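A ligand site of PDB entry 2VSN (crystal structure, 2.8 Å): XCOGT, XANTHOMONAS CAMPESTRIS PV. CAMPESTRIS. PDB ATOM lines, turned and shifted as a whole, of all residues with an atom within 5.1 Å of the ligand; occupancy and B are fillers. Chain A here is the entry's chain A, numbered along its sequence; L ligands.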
ATOM      1  N   HIS A 218      -8.624  -2.243   4.841  1.00  0.00           N
ATOM      2  CA  HIS A 218      -8.695  -2.633   6.236  1.00  0.00           C
ATOM      3  C   HIS A 218      -7.270  -3.114   6.524  1.00  0.00           C
ATOM      4  O   HIS A 218      -6.580  -3.590   5.635  1.00  0.00           O
ATOM      5  CB  HIS A 218      -9.733  -3.746   6.380  1.00  0.00           C
ATOM      6  CG  HIS A 218      -9.801  -4.358   7.742  1.00  0.00           C
ATOM      7  ND1 HIS A 218      -8.761  -5.083   8.295  1.00  0.00           N
ATOM      8  CD2 HIS A 218     -10.811  -4.419   8.643  1.00  0.00           C
ATOM      9  CE1 HIS A 218      -9.138  -5.579   9.460  1.00  0.00           C
ATOM     10  NE2 HIS A 218     -10.378  -5.190   9.698  1.00  0.00           N
ATOM     11  N   PRO A 219      -6.808  -2.971   7.770  1.00  0.00           N
ATOM     12  CA  PRO A 219      -5.441  -3.399   8.123  1.00  0.00           C
ATOM     13  C   PRO A 219      -5.006  -4.725   7.512  1.00  0.00           C
ATOM     14  O   PRO A 219      -3.967  -4.792   6.826  1.00  0.00           O
ATOM     15  CB  PRO A 219      -5.476  -3.453   9.631  1.00  0.00           C
ATOM     16  CG  PRO A 219      -6.387  -2.339   9.956  1.00  0.00           C
ATOM     17  CD  PRO A 219      -7.508  -2.490   8.966  1.00  0.00           C
ATOM     18  N   LEU A 222      -4.462  -4.658   3.839  1.00  0.00           N
ATOM     19  CA  LEU A 222      -3.361  -3.719   3.625  1.00  0.00           C
ATOM     20  C   LEU A 222      -1.991  -4.324   3.935  1.00  0.00           C
ATOM     21  O   LEU A 222      -1.000  -4.015   3.266  1.00  0.00           O
ATOM     22  CB  LEU A 222      -3.609  -2.477   4.469  1.00  0.00           C
ATOM     23  CG  LEU A 222      -2.647  -1.287   4.389  1.00  0.00           C
ATOM     24  CD1 LEU A 222      -2.523  -0.776   2.959  1.00  0.00           C
ATOM     25  CD2 LEU A 222      -3.186  -0.199   5.297  1.00  0.00           C
ATOM     26  N   ASN A 384      -2.651   6.852  16.289  1.00  0.00           N
ATOM     27  CA  ASN A 384      -3.308   5.653  16.756  1.00  0.00           C
ATOM     28  C   ASN A 384      -4.774   5.822  17.065  1.00  0.00           C
ATOM     29  O   ASN A 384      -5.237   6.935  17.303  1.00  0.00           O
ATOM     30  CB  ASN A 384      -2.599   5.100  17.985  1.00  0.00           C
ATOM     31  CG  ASN A 384      -1.303   4.422  17.644  1.00  0.00           C
ATOM     32  OD1 ASN A 384      -1.131   3.915  16.530  1.00  0.00           O
ATOM     33  ND2 ASN A 384      -0.370   4.381  18.587  1.00  0.00           N
ATOM     34  N   ASN A 385      -5.495   4.712  17.033  1.00  0.00           N
ATOM     35  CA  ASN A 385      -6.921   4.714  17.337  1.00  0.00           C
ATOM     36  C   ASN A 385      -7.110   5.282  18.746  1.00  0.00           C
ATOM     37  O   ASN A 385      -6.258   5.088  19.622  1.00  0.00           O
ATOM     38  CB  ASN A 385      -7.446   3.280  17.263  1.00  0.00           C
ATOM     39  CG  ASN A 385      -8.677   3.179  16.413  1.00  0.00           C
ATOM     40  OD1 ASN A 385      -9.630   3.944  16.590  1.00  0.00           O
ATOM     41  ND2 ASN A 385      -8.679   2.225  15.483  1.00  0.00           N
ATOM     42  N   TYR A 387      -8.809   4.453  21.429  1.00  0.00           N
ATOM     43  CA  TYR A 387      -8.747   3.573  22.594  1.00  0.00           C
ATOM     44  C   TYR A 387      -7.312   3.237  23.034  1.00  0.00           C
ATOM     45  O   TYR A 387      -7.088   2.796  24.159  1.00  0.00           O
ATOM     46  CB  TYR A 387      -9.553   2.286  22.355  1.00  0.00           C
ATOM     47  CG  TYR A 387      -9.238   1.549  21.076  1.00  0.00           C
ATOM     48  CD1 TYR A 387     -10.021   1.722  19.939  1.00  0.00           C
ATOM     49  CD2 TYR A 387      -8.173   0.647  21.020  1.00  0.00           C
ATOM     50  CE1 TYR A 387      -9.747   1.007  18.762  1.00  0.00           C
ATOM     51  CE2 TYR A 387      -7.890  -0.078  19.857  1.00  0.00           C
ATOM     52  CZ  TYR A 387      -8.674   0.113  18.719  1.00  0.00           C
ATOM     53  OH  TYR A 387      -8.369  -0.604  17.575  1.00  0.00           O
ATOM     54  N   LYS A 388      -6.341   3.465  22.152  1.00  0.00           N
ATOM     55  CA  LYS A 388      -4.933   3.222  22.466  1.00  0.00           C
ATOM     56  C   LYS A 388      -4.334   4.451  23.176  1.00  0.00           C
ATOM     57  O   LYS A 388      -3.222   4.402  23.720  1.00  0.00           O
ATOM     58  CB  LYS A 388      -4.134   2.961  21.188  1.00  0.00           C
ATOM     59  CG  LYS A 388      -4.511   1.707  20.462  1.00  0.00           C
ATOM     60  CD  LYS A 388      -3.646   1.551  19.242  1.00  0.00           C
ATOM     61  CE  LYS A 388      -3.941   0.272  18.511  1.00  0.00           C
ATOM     62  NZ  LYS A 388      -3.076   0.153  17.316  1.00  0.00           N
ATOM     63  N   LEU A 412      -4.856  11.608  15.545  1.00  0.00           N
ATOM     64  CA  LEU A 412      -5.951  11.200  14.679  1.00  0.00           C
ATOM     65  C   LEU A 412      -7.232  11.555  15.414  1.00  0.00           C
ATOM     66  O   LEU A 412      -7.480  11.042  16.505  1.00  0.00           O
ATOM     67  CB  LEU A 412      -5.901   9.694  14.406  1.00  0.00           C
ATOM     68  CG  LEU A 412      -6.995   9.187  13.455  1.00  0.00           C
ATOM     69  CD1 LEU A 412      -6.856   9.872  12.096  1.00  0.00           C
ATOM     70  CD2 LEU A 412      -6.898   7.691  13.299  1.00  0.00           C
ATOM     71  N   MET A 439      -6.277  15.341  13.022  1.00  0.00           N
ATOM     72  CA  MET A 439      -6.525  15.023  11.615  1.00  0.00           C
ATOM     73  C   MET A 439      -7.716  14.101  11.465  1.00  0.00           C
ATOM     74  O   MET A 439      -7.886  13.151  12.235  1.00  0.00           O
ATOM     75  CB  MET A 439      -5.290  14.357  11.001  1.00  0.00           C
ATOM     76  CG  MET A 439      -5.537  13.690   9.657  1.00  0.00           C
ATOM     77  SD  MET A 439      -4.089  12.778   9.100  1.00  0.00           S
ATOM     78  CE  MET A 439      -4.225  11.229  10.056  1.00  0.00           C
ATOM     79  N   PRO A 440      -8.585  14.379  10.477  1.00  0.00           N
ATOM     80  CA  PRO A 440      -9.782  13.550  10.257  1.00  0.00           C
ATOM     81  C   PRO A 440      -9.330  12.271   9.570  1.00  0.00           C
ATOM     82  O   PRO A 440      -8.328  12.282   8.881  1.00  0.00           O
ATOM     83  CB  PRO A 440     -10.621  14.409   9.336  1.00  0.00           C
ATOM     84  CG  PRO A 440     -10.099  15.806   9.540  1.00  0.00           C
ATOM     85  CD  PRO A 440      -8.630  15.573   9.621  1.00  0.00           C
ATOM     86  N   LYS A 441     -10.052  11.171   9.772  1.00  0.00           N
ATOM     87  CA  LYS A 441      -9.681   9.918   9.104  1.00  0.00           C
ATOM     88  C   LYS A 441      -9.767  10.174   7.583  1.00  0.00           C
ATOM     89  O   LYS A 441     -10.785  10.666   7.075  1.00  0.00           O
ATOM     90  CB  LYS A 441     -10.638   8.800   9.526  1.00  0.00           C
ATOM     91  CG  LYS A 441     -10.538   7.504   8.692  1.00  0.00           C
ATOM     92  CD  LYS A 441      -9.702   6.388   9.349  1.00  0.00           C
ATOM     93  CE  LYS A 441     -10.460   5.666  10.464  1.00  0.00           C
ATOM     94  NZ  LYS A 441     -11.725   4.995  10.009  1.00  0.00           N
ATOM     95  N   LEU A 442      -8.683   9.864   6.876  1.00  0.00           N
ATOM     96  CA  LEU A 442      -8.629  10.069   5.432  1.00  0.00           C
ATOM     97  C   LEU A 442      -8.398   8.752   4.689  1.00  0.00           C
ATOM     98  O   LEU A 442      -8.010   7.743   5.296  1.00  0.00           O
ATOM     99  CB  LEU A 442      -7.477  11.001   5.094  1.00  0.00           C
ATOM    100  CG  LEU A 442      -7.457  12.440   5.579  1.00  0.00           C
ATOM    101  CD1 LEU A 442      -6.000  12.915   5.691  1.00  0.00           C
ATOM    102  CD2 LEU A 442      -8.250  13.317   4.639  1.00  0.00           C
ATOM    103  N   PRO A 443      -8.643   8.742   3.372  1.00  0.00           N
ATOM    104  CA  PRO A 443      -8.422   7.515   2.601  1.00  0.00           C
ATOM    105  C   PRO A 443      -6.926   7.205   2.721  1.00  0.00           C
ATOM    106  O   PRO A 443      -6.093   8.123   2.666  1.00  0.00           O
ATOM    107  CB  PRO A 443      -8.846   7.913   1.190  1.00  0.00           C
ATOM    108  CG  PRO A 443      -9.926   8.920   1.444  1.00  0.00           C
ATOM    109  CD  PRO A 443      -9.341   9.749   2.556  1.00  0.00           C
ATOM    110  N   HIS A 444      -6.574   5.929   2.867  1.00  0.00           N
ATOM    111  CA  HIS A 444      -5.188   5.524   3.039  1.00  0.00           C
ATOM    112  C   HIS A 444      -4.133   6.303   2.265  1.00  0.00           C
ATOM    113  O   HIS A 444      -3.182   6.810   2.837  1.00  0.00           O
ATOM    114  CB  HIS A 444      -5.003   4.041   2.760  1.00  0.00           C
ATOM    115  CG  HIS A 444      -3.708   3.488   3.271  1.00  0.00           C
ATOM    116  ND1 HIS A 444      -3.441   3.344   4.619  1.00  0.00           N
ATOM    117  CD2 HIS A 444      -2.603   3.079   2.620  1.00  0.00           C
ATOM    118  CE1 HIS A 444      -2.225   2.843   4.770  1.00  0.00           C
ATOM    119  NE2 HIS A 444      -1.694   2.678   3.578  1.00  0.00           N
ATOM    120  N   TYR A 447      -3.818   9.761   3.766  1.00  0.00           N
ATOM    121  CA  TYR A 447      -3.350   9.676   5.142  1.00  0.00           C
ATOM    122  C   TYR A 447      -1.852   9.374   5.140  1.00  0.00           C
ATOM    123  O   TYR A 447      -1.086   9.999   5.868  1.00  0.00           O
ATOM    124  CB  TYR A 447      -4.116   8.583   5.874  1.00  0.00           C
ATOM    125  CG  TYR A 447      -3.297   7.727   6.839  1.00  0.00           C
ATOM    126  CD1 TYR A 447      -2.949   8.184   8.106  1.00  0.00           C
ATOM    127  CD2 TYR A 447      -2.922   6.428   6.488  1.00  0.00           C
ATOM    128  CE1 TYR A 447      -2.257   7.362   9.001  1.00  0.00           C
ATOM    129  CE2 TYR A 447      -2.227   5.617   7.375  1.00  0.00           C
ATOM    130  CZ  TYR A 447      -1.901   6.083   8.621  1.00  0.00           C
ATOM    131  OH  TYR A 447      -1.219   5.253   9.489  1.00  0.00           O
ATOM    132  N   TYR A 463      -1.035  -0.767  24.141  1.00  0.00           N
ATOM    133  CA  TYR A 463      -1.448  -1.248  22.832  1.00  0.00           C
ATOM    134  C   TYR A 463      -0.727  -0.384  21.787  1.00  0.00           C
ATOM    135  O   TYR A 463      -1.137   0.747  21.521  1.00  0.00           O
ATOM    136  CB  TYR A 463      -2.959  -1.138  22.679  1.00  0.00           C
ATOM    137  CG  TYR A 463      -3.572  -1.953  21.540  1.00  0.00           C
ATOM    138  CD1 TYR A 463      -2.809  -2.303  20.422  1.00  0.00           C
ATOM    139  CD2 TYR A 463      -4.912  -2.309  21.559  1.00  0.00           C
ATOM    140  CE1 TYR A 463      -3.380  -2.977  19.354  1.00  0.00           C
ATOM    141  CE2 TYR A 463      -5.496  -2.983  20.499  1.00  0.00           C
ATOM    142  CZ  TYR A 463      -4.719  -3.314  19.400  1.00  0.00           C
ATOM    143  OH  TYR A 463      -5.309  -3.966  18.332  1.00  0.00           O
ATOM    144  N   ASN A 464       0.354  -0.909  21.225  1.00  0.00           N
ATOM    145  CA  ASN A 464       1.168  -0.186  20.240  1.00  0.00           C
ATOM    146  C   ASN A 464       0.413   0.107  18.971  1.00  0.00           C
ATOM    147  O   ASN A 464      -0.714  -0.319  18.764  1.00  0.00           O
ATOM    148  CB  ASN A 464       2.392  -1.004  19.795  1.00  0.00           C
ATOM    149  CG  ASN A 464       3.363  -1.309  20.905  1.00  0.00           C
ATOM    150  OD1 ASN A 464       3.105  -1.012  22.056  1.00  0.00           O
ATOM    151  ND2 ASN A 464       4.487  -1.916  20.551  1.00  0.00           N
ATOM    152  N   ALA A 465       1.098   0.838  18.111  1.00  0.00           N
ATOM    153  CA  ALA A 465       0.570   1.110  16.796  1.00  0.00           C
ATOM    154  C   ALA A 465       1.119  -0.147  16.114  1.00  0.00           C
ATOM    155  O   ALA A 465       2.267  -0.540  16.375  1.00  0.00           O
ATOM    156  CB  ALA A 465       1.221   2.348  16.234  1.00  0.00           C
ATOM    157  N   HIS A 466       0.326  -0.821  15.285  1.00  0.00           N
ATOM    158  CA  HIS A 466       0.819  -2.005  14.595  1.00  0.00           C
ATOM    159  C   HIS A 466       0.857  -1.688  13.116  1.00  0.00           C
ATOM    160  O   HIS A 466       1.907  -1.403  12.558  1.00  0.00           O
ATOM    161  CB  HIS A 466      -0.078  -3.214  14.855  1.00  0.00           C
ATOM    162  CG  HIS A 466      -0.119  -3.633  16.293  1.00  0.00           C
ATOM    163  ND1 HIS A 466      -0.840  -4.720  16.743  1.00  0.00           N
ATOM    164  CD2 HIS A 466       0.482  -3.106  17.391  1.00  0.00           C
ATOM    165  CE1 HIS A 466      -0.680  -4.849  18.049  1.00  0.00           C
ATOM    166  NE2 HIS A 466       0.122  -3.886  18.470  1.00  0.00           N
ATOM    167  N   THR A 467      -0.296  -1.734  12.475  1.00  0.00           N
ATOM    168  CA  THR A 467      -0.326  -1.397  11.071  1.00  0.00           C
ATOM    169  C   THR A 467       0.102   0.048  10.967  1.00  0.00           C
ATOM    170  O   THR A 467       0.800   0.422  10.040  1.00  0.00           O
ATOM    171  CB  THR A 467      -1.740  -1.557  10.490  1.00  0.00           C
ATOM    172  OG1 THR A 467      -2.131  -2.929  10.536  1.00  0.00           O
ATOM    173  CG2 THR A 467      -1.740  -1.116   9.054  1.00  0.00           C
ATOM    174  N   THR A 468      -0.306   0.881  11.941  1.00  0.00           N
ATOM    175  CA  THR A 468       0.046   2.295  11.938  1.00  0.00           C
ATOM    176  C   THR A 468       1.541   2.522  12.116  1.00  0.00           C
ATOM    177  O   THR A 468       2.096   3.497  11.589  1.00  0.00           O
ATOM    178  CB  THR A 468      -0.644   3.079  13.074  1.00  0.00           C
ATOM    179  OG1 THR A 468      -1.982   2.601  13.244  1.00  0.00           O
ATOM    180  CG2 THR A 468      -0.700   4.548  12.745  1.00  0.00           C
ATOM    181  N   ASP A 471       3.097   1.833   8.808  1.00  0.00           N
ATOM    182  CA  ASP A 471       2.680   2.823   7.813  1.00  0.00           C
ATOM    183  C   ASP A 471       3.708   3.959   7.903  1.00  0.00           C
ATOM    184  O   ASP A 471       4.244   4.411   6.891  1.00  0.00           O
ATOM    185  CB  ASP A 471       1.306   3.414   8.117  1.00  0.00           C
ATOM    186  CG  ASP A 471       0.168   2.485   7.771  1.00  0.00           C
ATOM    187  OD1 ASP A 471       0.283   1.703   6.811  1.00  0.00           O
ATOM    188  OD2 ASP A 471      -0.872   2.587   8.455  1.00  0.00           O
HETATM  189  N1  LIG L   1      -5.835   4.643   8.505  1.00  0.00           N
HETATM  190  C1  LIG L   1      -6.185   5.271   7.348  1.00  0.00           C
HETATM  191  N2  LIG L   1      -6.422   6.620   7.328  1.00  0.00           N
HETATM  192  C2  LIG L   1      -6.308   7.360   8.493  1.00  0.00           C
HETATM  193  C3  LIG L   1      -5.961   6.720   9.658  1.00  0.00           C
HETATM  194  C4  LIG L   1      -5.733   5.364   9.665  1.00  0.00           C
HETATM  195  O1  LIG L   1      -6.289   4.613   6.332  1.00  0.00           O
HETATM  196  O2  LIG L   1      -6.518   8.559   8.475  1.00  0.00           O
HETATM  197  C5  LIG L   1      -5.622   3.202   8.477  1.00  0.00           C
HETATM  198  C6  LIG L   1      -4.309   2.673   8.978  1.00  0.00           C
HETATM  199  O3  LIG L   1      -3.448   2.542   7.862  1.00  0.00           O
HETATM  200  C7  LIG L   1      -4.739   1.291   9.326  1.00  0.00           C
HETATM  201  C8  LIG L   1      -6.100   1.491   9.908  1.00  0.00           C
HETATM  202  O4  LIG L   1      -6.525   2.761   9.483  1.00  0.00           O
HETATM  203  O5  LIG L   1      -4.907   0.626   8.096  1.00  0.00           O
HETATM  204  C9  LIG L   1      -5.842   1.611  11.379  1.00  0.00           C
HETATM  205  O6  LIG L   1      -6.309   0.483  12.046  1.00  0.00           O
HETATM  206  P1  LIG L   1      -5.933   0.183  13.475  1.00  0.00           P
HETATM  207  O7  LIG L   1      -7.152  -0.584  13.977  1.00  0.00           O
HETATM  208  O8  LIG L   1      -5.643   1.334  14.287  1.00  0.00           O
HETATM  209  O9  LIG L   1      -4.831  -0.906  13.289  1.00  0.00           O
HETATM  210  P2  LIG L   1      -3.462  -1.156  14.005  1.00  0.00           P
HETATM  211  O10 LIG L   1      -3.773  -1.733  15.377  1.00  0.00           O
HETATM  212  O11 LIG L   1      -2.739   0.156  14.249  1.00  0.00           O
HETATM  213  O12 LIG L   1      -2.702  -2.079  13.215  1.00  0.00           O
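O11 of the ligand lies within hydrogen-bond range of N of His 466 (3.4 Å).
O10 of the ligand lies within salt-bridge range of NZ of Lys 388.
OG1 of Thr 468 is in hydrogen-bond range of O11 of the ligand.
A ring nitrogen (ND1) of His 444 lies close to an oxygen (O3) of the ligand, at 3.3 Å.
The side-chain hydroxyl of Thr 467 lies within hydrogen-bond range of an oxygen (O12) of the ligand, at 2.9 Å.
An oxygen (O8) of the ligand is in hydrogen-bond range of the side-chain amide nitrogen (ND2) of Asn 385, 3.4 Å away.
N of Thr 468 lies within hydrogen-bond range of O11 of the ligand (3.4 Å).
The side-chain carboxylate (OD2) of Asp 471 lies within hydrogen-bond range of an oxygen (O3) of the ligand (2.6 Å).
O of Leu 442 lies within hydrogen-bond range of N2 of the ligand, at 2.8 Å.
N of Thr 467 lies within hydrogen-bond range of O12 of the ligand, at 2.5 Å.
An oxygen (O2) of the ligand sits at hydrogen-bond distance from the backbone NH of Leu 442 (3.0 Å).
The backbone carbonyl oxygen (O) of Asn 464 sits at hydrogen-bond distance from the side-chain amino group (NZ) of Lys 388, at 2.8 Å.
The side-chain hydroxyl (OH) of Tyr 447 lies within hydrogen-bond range of the side-chain carboxylate (OD2) of Asp 471.
Residues that only touch the ligand: Pro 219, Leu 222, Tyr 387, Leu 412, Met 439, Lys 441 and Tyr 447.
Hydrophobic or aromatic side chains that line the ligand: Pro 219, Leu 222, Leu 412, Met 439, His 444, Tyr 447 and His 466.
Of the 22 residues printed, 15 come within 4 Å of the ligand.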
